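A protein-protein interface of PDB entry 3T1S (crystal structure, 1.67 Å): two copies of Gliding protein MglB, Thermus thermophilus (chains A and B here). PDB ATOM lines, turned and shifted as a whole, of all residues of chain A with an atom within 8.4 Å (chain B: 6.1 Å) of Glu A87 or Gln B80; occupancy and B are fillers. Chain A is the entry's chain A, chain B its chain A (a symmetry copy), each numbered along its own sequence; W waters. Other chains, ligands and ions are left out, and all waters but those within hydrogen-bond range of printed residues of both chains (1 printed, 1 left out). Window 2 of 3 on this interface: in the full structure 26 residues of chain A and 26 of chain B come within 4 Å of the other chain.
No position is printed for both chains.
Printed residues of chain B that touch a printed residue of chain A: Glu B76, Phe B79, Gln B80, Glu B81 and Glu B82. Hydrophobic or aromatic side chains of chain B within 4 Å of the printed part of chain A: Phe B79.
The side-chain sulfur (SD) of Met A89 sits close to the guanidinium group (NH1) of Arg A88, 3.5 Å away. N of Glu A108 sits at hydrogen-bond distance from O of Arg A88 (3.3 Å). The backbone carbonyl oxygen (O) of Gln B80 lies within hydrogen-bond range of the backbone NH (N) of Glu B95 (2.9 Å). N of Glu B82 is in hydrogen-bond range of O of Val B93 (2.9 Å).
Among the printed residues, merely in contact across the chains: Val A83 with Glu B82 (3.2 Å), His A84 with Phe B79 (3.8 Å), His A84 with Glu B81 (3.6 Å), Gln A85 with Phe B79 (3.6 Å), Gly A86 with Glu B76 (3.7 Å), Gly A86 with Phe B79 (3.9 Å), Gly A86 with Gln B80 (3.5 Å), Glu A87 with Glu B76 (3.7 Å), Glu A87 with Gln B80 (3.4 Å) and Arg A88 with Glu B76 (3.9 Å).
Water W1 bridges OE2 of Glu B81 (2.6 Å) and NE2 of Gln A85 (2.7 Å).
Printed residues of chain B within 4 Å of Glu A87: Glu B76 (3.7 Å) and Gln B80 (3.4 Å). Gln B80 touches three residues of chain A. Of the printed residues of chain B, His A84 touches Phe B79, Glu B81 and Glu B82. Of the printed residues of chain B, Arg A88 touches Glu B76. Of the printed residues of chain A, Glu B76 touches Gly A86 (3.7 Å), Glu A87 (3.7 Å), Arg A88 (3.9 Å) and Met A89 (3.4 Å). Of the printed residues of chain B, Gln A85 touches Phe B79 (3.6 Å), Gln B80 (2.7 Å) and Glu B81 (2.8 Å). Of the printed residues of chain B, Gly A86 touches Glu B76 (3.7 Å), Phe B79 (3.9 Å) and Gln B80 (3.5 Å). Leu B101 touches none of the printed residues of chain A. Glu A108 touches none of the printed residues of chain B.
A ring nitrogen (NE2) of His A84 sits at hydrogen-bond distance from the side-chain carboxylate of Glu B82, 3.3 Å away. The backbone carbonyl oxygen (O) of Gln A85 is in hydrogen-bond range of the backbone NH (N) of Gln B80. The backbone carbonyl oxygen (O) of Glu B81 sits at hydrogen-bond distance from the backbone NH (N) of Gln A85 (2.8 Å). The side-chain carboxylate (OE1) of Glu B76 sits at hydrogen-bond distance from the backbone NH (N) of Met A89, 3.4 Å away.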
ATOM      1  N   VAL A  83      -0.156   8.427  11.449  1.00  0.00           N
ATOM      2  CA  VAL A  83       0.362   8.953  10.147  1.00  0.00           C
ATOM      3  C   VAL A  83      -0.792   9.646   9.468  1.00  0.00           C
ATOM      4  O   VAL A  83      -1.938   9.085   9.397  1.00  0.00           O
ATOM      5  CB  VAL A  83       0.863   7.833   9.278  1.00  0.00           C
ATOM      6  CG1 VAL A  83       1.224   8.440   7.899  1.00  0.00           C
ATOM      7  CG2 VAL A  83       2.221   7.239   9.863  1.00  0.00           C
ATOM      8  N   HIS A  84      -0.616  10.855   8.929  1.00  0.00           N
ATOM      9  CA  HIS A  84      -1.679  11.494   8.198  1.00  0.00           C
ATOM     10  C   HIS A  84      -1.042  11.832   6.823  1.00  0.00           C
ATOM     11  O   HIS A  84       0.078  12.400   6.741  1.00  0.00           O
ATOM     12  CB  HIS A  84      -2.086  12.832   8.834  1.00  0.00           C
ATOM     13  CG  HIS A  84      -2.690  12.682  10.192  1.00  0.00           C
ATOM     14  ND1 HIS A  84      -1.939  12.438  11.320  1.00  0.00           N
ATOM     15  CD2 HIS A  84      -3.977  12.713  10.590  1.00  0.00           C
ATOM     16  CE1 HIS A  84      -2.750  12.303  12.352  1.00  0.00           C
ATOM     17  NE2 HIS A  84      -3.993  12.471  11.933  1.00  0.00           N
ATOM     18  N   GLN A  85      -1.712  11.413   5.764  1.00  0.00           N
ATOM     19  CA  GLN A  85      -1.092  11.631   4.405  1.00  0.00           C
ATOM     20  C   GLN A  85      -1.997  12.427   3.499  1.00  0.00           C
ATOM     21  O   GLN A  85      -3.212  12.171   3.383  1.00  0.00           O
ATOM     22  CB  GLN A  85      -0.706  10.345   3.691  1.00  0.00           C
ATOM     23  CG  GLN A  85       0.253   9.497   4.489  1.00  0.00           C
ATOM     24  CD  GLN A  85       0.772   8.367   3.686  1.00  0.00           C
ATOM     25  OE1 GLN A  85       1.515   8.614   2.721  1.00  0.00           O
ATOM     26  NE2 GLN A  85       0.429   7.128   4.048  1.00  0.00           N
ATOM     27  N   GLY A  86      -1.419  13.472   2.900  1.00  0.00           N
ATOM     28  CA  GLY A  86      -2.143  14.252   1.886  1.00  0.00           C
ATOM     29  C   GLY A  86      -1.549  13.848   0.536  1.00  0.00           C
ATOM     30  O   GLY A  86      -0.968  12.763   0.378  1.00  0.00           O
ATOM     31  N   GLU A  87      -1.844  14.623  -0.489  1.00  0.00           N
ATOM     32  CA  GLU A  87      -1.398  14.252  -1.831  1.00  0.00           C
ATOM     33  C   GLU A  87       0.118  14.323  -1.940  1.00  0.00           C
ATOM     34  O   GLU A  87       0.765  13.402  -2.523  1.00  0.00           O
ATOM     35  CB  GLU A  87      -1.966  15.243  -2.807  1.00  0.00           C
ATOM     36  CG  GLU A  87      -3.282  14.909  -3.288  1.00  0.00           C
ATOM     37  CD  GLU A  87      -3.564  15.707  -4.534  1.00  0.00           C
ATOM     38  OE1 GLU A  87      -2.604  16.350  -5.061  1.00  0.00           O
ATOM     39  OE2 GLU A  87      -4.746  15.691  -4.925  1.00  0.00           O
ATOM     40  N   ARG A  88       0.642  15.384  -1.340  1.00  0.00           N
ATOM     41  CA  ARG A  88       2.074  15.632  -1.298  1.00  0.00           C
ATOM     42  C   ARG A  88       2.706  15.463   0.095  1.00  0.00           C
ATOM     43  O   ARG A  88       3.702  14.732   0.203  1.00  0.00           O
ATOM     44  CB  ARG A  88       2.426  16.985  -1.942  1.00  0.00           C
ATOM     45  CG  ARG A  88       1.873  18.276  -1.307  1.00  0.00           C
ATOM     46  CD  ARG A  88       2.750  19.451  -1.760  1.00  0.00           C
ATOM     47  NE  ARG A  88       1.998  20.698  -1.790  1.00  0.00           N
ATOM     48  CZ  ARG A  88       1.984  21.572  -0.795  1.00  0.00           C
ATOM     49  NH1 ARG A  88       2.691  21.328   0.299  1.00  0.00           N
ATOM     50  NH2 ARG A  88       1.269  22.678  -0.890  1.00  0.00           N
ATOM     51  N   MET A  89       2.064  16.059   1.127  1.00  0.00           N
ATOM     52  CA  MET A  89       2.675  16.282   2.490  1.00  0.00           C
ATOM     53  C   MET A  89       2.125  15.168   3.409  1.00  0.00           C
ATOM     54  O   MET A  89       0.999  14.670   3.197  1.00  0.00           O
ATOM     55  CB  MET A  89       2.283  17.623   3.114  1.00  0.00           C
ATOM     56  CG  MET A  89       2.852  18.930   2.522  1.00  0.00           C
ATOM     57  SD  MET A  89       4.622  19.057   2.116  1.00  0.00           S
ATOM     58  CE  MET A  89       5.510  18.382   3.534  1.00  0.00           C
ATOM     59  N   GLY A  90       2.909  14.711   4.365  1.00  0.00           N
ATOM     60  CA  GLY A  90       2.374  13.793   5.369  1.00  0.00           C
ATOM     61  C   GLY A  90       2.978  14.212   6.701  1.00  0.00           C
ATOM     62  O   GLY A  90       3.892  15.084   6.807  1.00  0.00           O
ATOM     63  N   PHE A 106       6.867  15.440   6.209  1.00  0.00           N
ATOM     64  CA  PHE A 106       7.621  14.960   5.040  1.00  0.00           C
ATOM     65  C   PHE A 106       6.799  15.086   3.767  1.00  0.00           C
ATOM     66  O   PHE A 106       5.622  15.401   3.802  1.00  0.00           O
ATOM     67  CB  PHE A 106       8.033  13.517   5.281  1.00  0.00           C
ATOM     68  CG  PHE A 106       6.842  12.570   5.503  1.00  0.00           C
ATOM     69  CD1 PHE A 106       6.337  11.822   4.430  1.00  0.00           C
ATOM     70  CD2 PHE A 106       6.207  12.438   6.766  1.00  0.00           C
ATOM     71  CE1 PHE A 106       5.243  10.947   4.597  1.00  0.00           C
ATOM     72  CE2 PHE A 106       5.107  11.602   6.916  1.00  0.00           C
ATOM     73  CZ  PHE A 106       4.580  10.888   5.830  1.00  0.00           C
ATOM     74  N   ASP A 107       7.500  14.991   2.635  1.00  0.00           N
ATOM     75  CA  ASP A 107       6.783  14.998   1.317  1.00  0.00           C
ATOM     76  C   ASP A 107       7.036  13.649   0.617  1.00  0.00           C
ATOM     77  O   ASP A 107       7.592  12.712   1.183  1.00  0.00           O
ATOM     78  CB  ASP A 107       7.324  16.175   0.469  1.00  0.00           C
ATOM     79  CG  ASP A 107       8.813  16.093   0.222  1.00  0.00           C
ATOM     80  OD1 ASP A 107       9.406  17.206   0.241  1.00  0.00           O
ATOM     81  OD2 ASP A 107       9.398  15.000  -0.002  1.00  0.00           O
ATOM     82  N   GLU A 108       6.662  13.546  -0.688  1.00  0.00           N
ATOM     83  CA  GLU A 108       6.746  12.265  -1.423  1.00  0.00           C
ATOM     84  C   GLU A 108       8.132  11.698  -1.649  1.00  0.00           C
ATOM     85  O   GLU A 108       8.286  10.486  -1.967  1.00  0.00           O
ATOM     86  CB  GLU A 108       6.062  12.387  -2.791  1.00  0.00           C
ATOM     87  CG  GLU A 108       6.821  13.270  -3.808  1.00  0.00           C
ATOM     88  CD  GLU A 108       6.001  13.490  -5.052  1.00  0.00           C
ATOM     89  OE1 GLU A 108       4.940  12.826  -5.195  1.00  0.00           O
ATOM     90  OE2 GLU A 108       6.387  14.349  -5.864  1.00  0.00           O
ATOM     91  N   GLU B  76      -1.649  21.951   2.489  1.00  0.00           N
ATOM     92  CA  GLU B  76      -2.543  21.276   1.554  1.00  0.00           C
ATOM     93  C   GLU B  76      -3.951  21.393   2.030  1.00  0.00           C
ATOM     94  O   GLU B  76      -4.208  21.921   3.124  1.00  0.00           O
ATOM     95  CB  GLU B  76      -2.174  19.842   1.333  1.00  0.00           C
ATOM     96  CG  GLU B  76      -2.467  18.970   2.517  1.00  0.00           C
ATOM     97  CD  GLU B  76      -1.445  17.915   2.535  1.00  0.00           C
ATOM     98  OE1 GLU B  76      -0.937  17.672   1.415  1.00  0.00           O
ATOM     99  OE2 GLU B  76      -1.148  17.370   3.641  1.00  0.00           O
ATOM    100  N   ARG B  78      -6.531  19.122   2.579  1.00  0.00           N
ATOM    101  CA  ARG B  78      -7.000  18.177   3.609  1.00  0.00           C
ATOM    102  C   ARG B  78      -6.090  16.968   3.592  1.00  0.00           C
ATOM    103  O   ARG B  78      -5.361  16.770   2.632  1.00  0.00           O
ATOM    104  CB  ARG B  78      -8.466  17.753   3.334  1.00  0.00           C
ATOM    105  CG  ARG B  78      -8.820  17.540   1.863  1.00  0.00           C
ATOM    106  CD  ARG B  78     -10.295  17.065   1.729  1.00  0.00           C
ATOM    107  NE  ARG B  78     -10.409  15.886   0.870  1.00  0.00           N
ATOM    108  CZ  ARG B  78     -11.561  15.337   0.479  1.00  0.00           C
ATOM    109  NH1 ARG B  78     -12.723  15.863   0.859  1.00  0.00           N
ATOM    110  NH2 ARG B  78     -11.540  14.258  -0.297  1.00  0.00           N
ATOM    111  N   PHE B  79      -6.128  16.120   4.624  1.00  0.00           N
ATOM    112  CA  PHE B  79      -5.422  14.836   4.455  1.00  0.00           C
ATOM    113  C   PHE B  79      -6.354  13.855   3.701  1.00  0.00           C
ATOM    114  O   PHE B  79      -7.598  14.023   3.741  1.00  0.00           O
ATOM    115  CB  PHE B  79      -5.116  14.284   5.855  1.00  0.00           C
ATOM    116  CG  PHE B  79      -4.088  15.090   6.580  1.00  0.00           C
ATOM    117  CD1 PHE B  79      -2.820  15.229   6.028  1.00  0.00           C
ATOM    118  CD2 PHE B  79      -4.367  15.637   7.779  1.00  0.00           C
ATOM    119  CE1 PHE B  79      -1.818  16.007   6.714  1.00  0.00           C
ATOM    120  CE2 PHE B  79      -3.353  16.371   8.530  1.00  0.00           C
ATOM    121  CZ  PHE B  79      -2.095  16.526   7.910  1.00  0.00           C
ATOM    122  N   GLN B  80      -5.803  12.894   3.013  1.00  0.00           N
ATOM    123  CA  GLN B  80      -6.656  11.951   2.293  1.00  0.00           C
ATOM    124  C   GLN B  80      -6.792  10.647   3.083  1.00  0.00           C
ATOM    125  O   GLN B  80      -7.780   9.920   2.924  1.00  0.00           O
ATOM    126  CB  GLN B  80      -5.968  11.581   1.029  1.00  0.00           C
ATOM    127  CG  GLN B  80      -5.779  12.833   0.137  1.00  0.00           C
ATOM    128  CD  GLN B  80      -5.147  12.468  -1.175  1.00  0.00           C
ATOM    129  OE1 GLN B  80      -5.701  12.748  -2.246  1.00  0.00           O
ATOM    130  NE2 GLN B  80      -4.000  11.811  -1.115  1.00  0.00           N
ATOM    131  N   GLU B  81      -5.773  10.350   3.883  1.00  0.00           N
ATOM    132  CA  GLU B  81      -5.717   9.033   4.547  1.00  0.00           C
ATOM    133  C   GLU B  81      -5.079   9.225   5.930  1.00  0.00           C
ATOM    134  O   GLU B  81      -4.197  10.062   6.065  1.00  0.00           O
ATOM    135  CB  GLU B  81      -4.942   8.047   3.690  1.00  0.00           C
ATOM    136  CG  GLU B  81      -4.964   6.568   4.129  1.00  0.00           C
ATOM    137  CD  GLU B  81      -3.676   6.161   4.871  1.00  0.00           C
ATOM    138  OE1 GLU B  81      -3.029   5.216   4.458  1.00  0.00           O
ATOM    139  OE2 GLU B  81      -3.278   6.814   5.835  1.00  0.00           O
ATOM    140  N   GLU B  82      -5.515   8.447   6.949  1.00  0.00           N
ATOM    141  CA  GLU B  82      -4.815   8.482   8.254  1.00  0.00           C
ATOM    142  C   GLU B  82      -4.850   7.119   8.897  1.00  0.00           C
ATOM    143  O   GLU B  82      -5.775   6.343   8.652  1.00  0.00           O
ATOM    144  CB  GLU B  82      -5.404   9.478   9.277  1.00  0.00           C
ATOM    145  CG  GLU B  82      -6.833   9.252   9.518  1.00  0.00           C
ATOM    146  CD  GLU B  82      -7.418  10.376  10.315  1.00  0.00           C
ATOM    147  OE1 GLU B  82      -8.500  10.854   9.941  1.00  0.00           O
ATOM    148  OE2 GLU B  82      -6.796  10.832  11.277  1.00  0.00           O
ATOM    149  N   VAL B  93      -8.414   5.334   8.142  1.00  0.00           N
ATOM    150  CA  VAL B  93      -9.490   6.056   7.555  1.00  0.00           C
ATOM    151  C   VAL B  93      -9.003   6.599   6.212  1.00  0.00           C
ATOM    152  O   VAL B  93      -7.918   7.168   6.097  1.00  0.00           O
ATOM    153  CB  VAL B  93      -9.916   7.257   8.446  1.00  0.00           C
ATOM    154  CG1 VAL B  93     -11.093   7.982   7.816  1.00  0.00           C
ATOM    155  CG2 VAL B  93     -10.223   6.798   9.909  1.00  0.00           C
ATOM    156  N   ASP B  94      -9.833   6.449   5.186  1.00  0.00           N
ATOM    157  CA  ASP B  94      -9.460   6.901   3.860  1.00  0.00           C
ATOM    158  C   ASP B  94     -10.656   7.679   3.286  1.00  0.00           C
ATOM    159  O   ASP B  94     -11.812   7.248   3.389  1.00  0.00           O
ATOM    160  CB  ASP B  94      -9.070   5.725   3.008  1.00  0.00           C
ATOM    161  CG  ASP B  94      -8.429   6.152   1.672  1.00  0.00           C
ATOM    162  OD1 ASP B  94      -7.731   7.168   1.642  1.00  0.00           O
ATOM    163  OD2 ASP B  94      -8.627   5.517   0.634  1.00  0.00           O
ATOM    164  N   GLU B  95     -10.403   8.798   2.603  1.00  0.00           N
ATOM    165  CA  GLU B  95     -11.463   9.507   1.872  1.00  0.00           C
ATOM    166  C   GLU B  95     -12.114   8.532   0.907  1.00  0.00           C
ATOM    167  O   GLU B  95     -11.393   7.788   0.210  1.00  0.00           O
ATOM    168  CB  GLU B  95     -10.821  10.668   1.077  1.00  0.00           C
ATOM    169  CG  GLU B  95     -11.789  11.512   0.198  1.00  0.00           C
ATOM    170  CD  GLU B  95     -11.683  11.311  -1.350  1.00  0.00           C
ATOM    171  OE1 GLU B  95     -11.449  10.174  -1.808  1.00  0.00           O
ATOM    172  OE2 GLU B  95     -11.888  12.283  -2.138  1.00  0.00           O
ATOM    173  N   LEU B 101     -16.227   8.593   4.129  1.00  0.00           N
ATOM    174  CA  LEU B 101     -14.933   8.074   4.606  1.00  0.00           C
ATOM    175  C   LEU B 101     -15.051   6.587   4.809  1.00  0.00           C
ATOM    176  O   LEU B 101     -16.119   6.141   5.291  1.00  0.00           O
ATOM    177  CB  LEU B 101     -14.603   8.701   5.963  1.00  0.00           C
ATOM    178  CG  LEU B 101     -14.521  10.251   5.972  1.00  0.00           C
ATOM    179  CD1 LEU B 101     -14.460  10.675   7.421  1.00  0.00           C
ATOM    180  CD2 LEU B 101     -13.241  10.580   5.342  1.00  0.00           C
HETATM  181  O   HOH W   1      -0.761   6.305   6.342  1.00  0.00           O
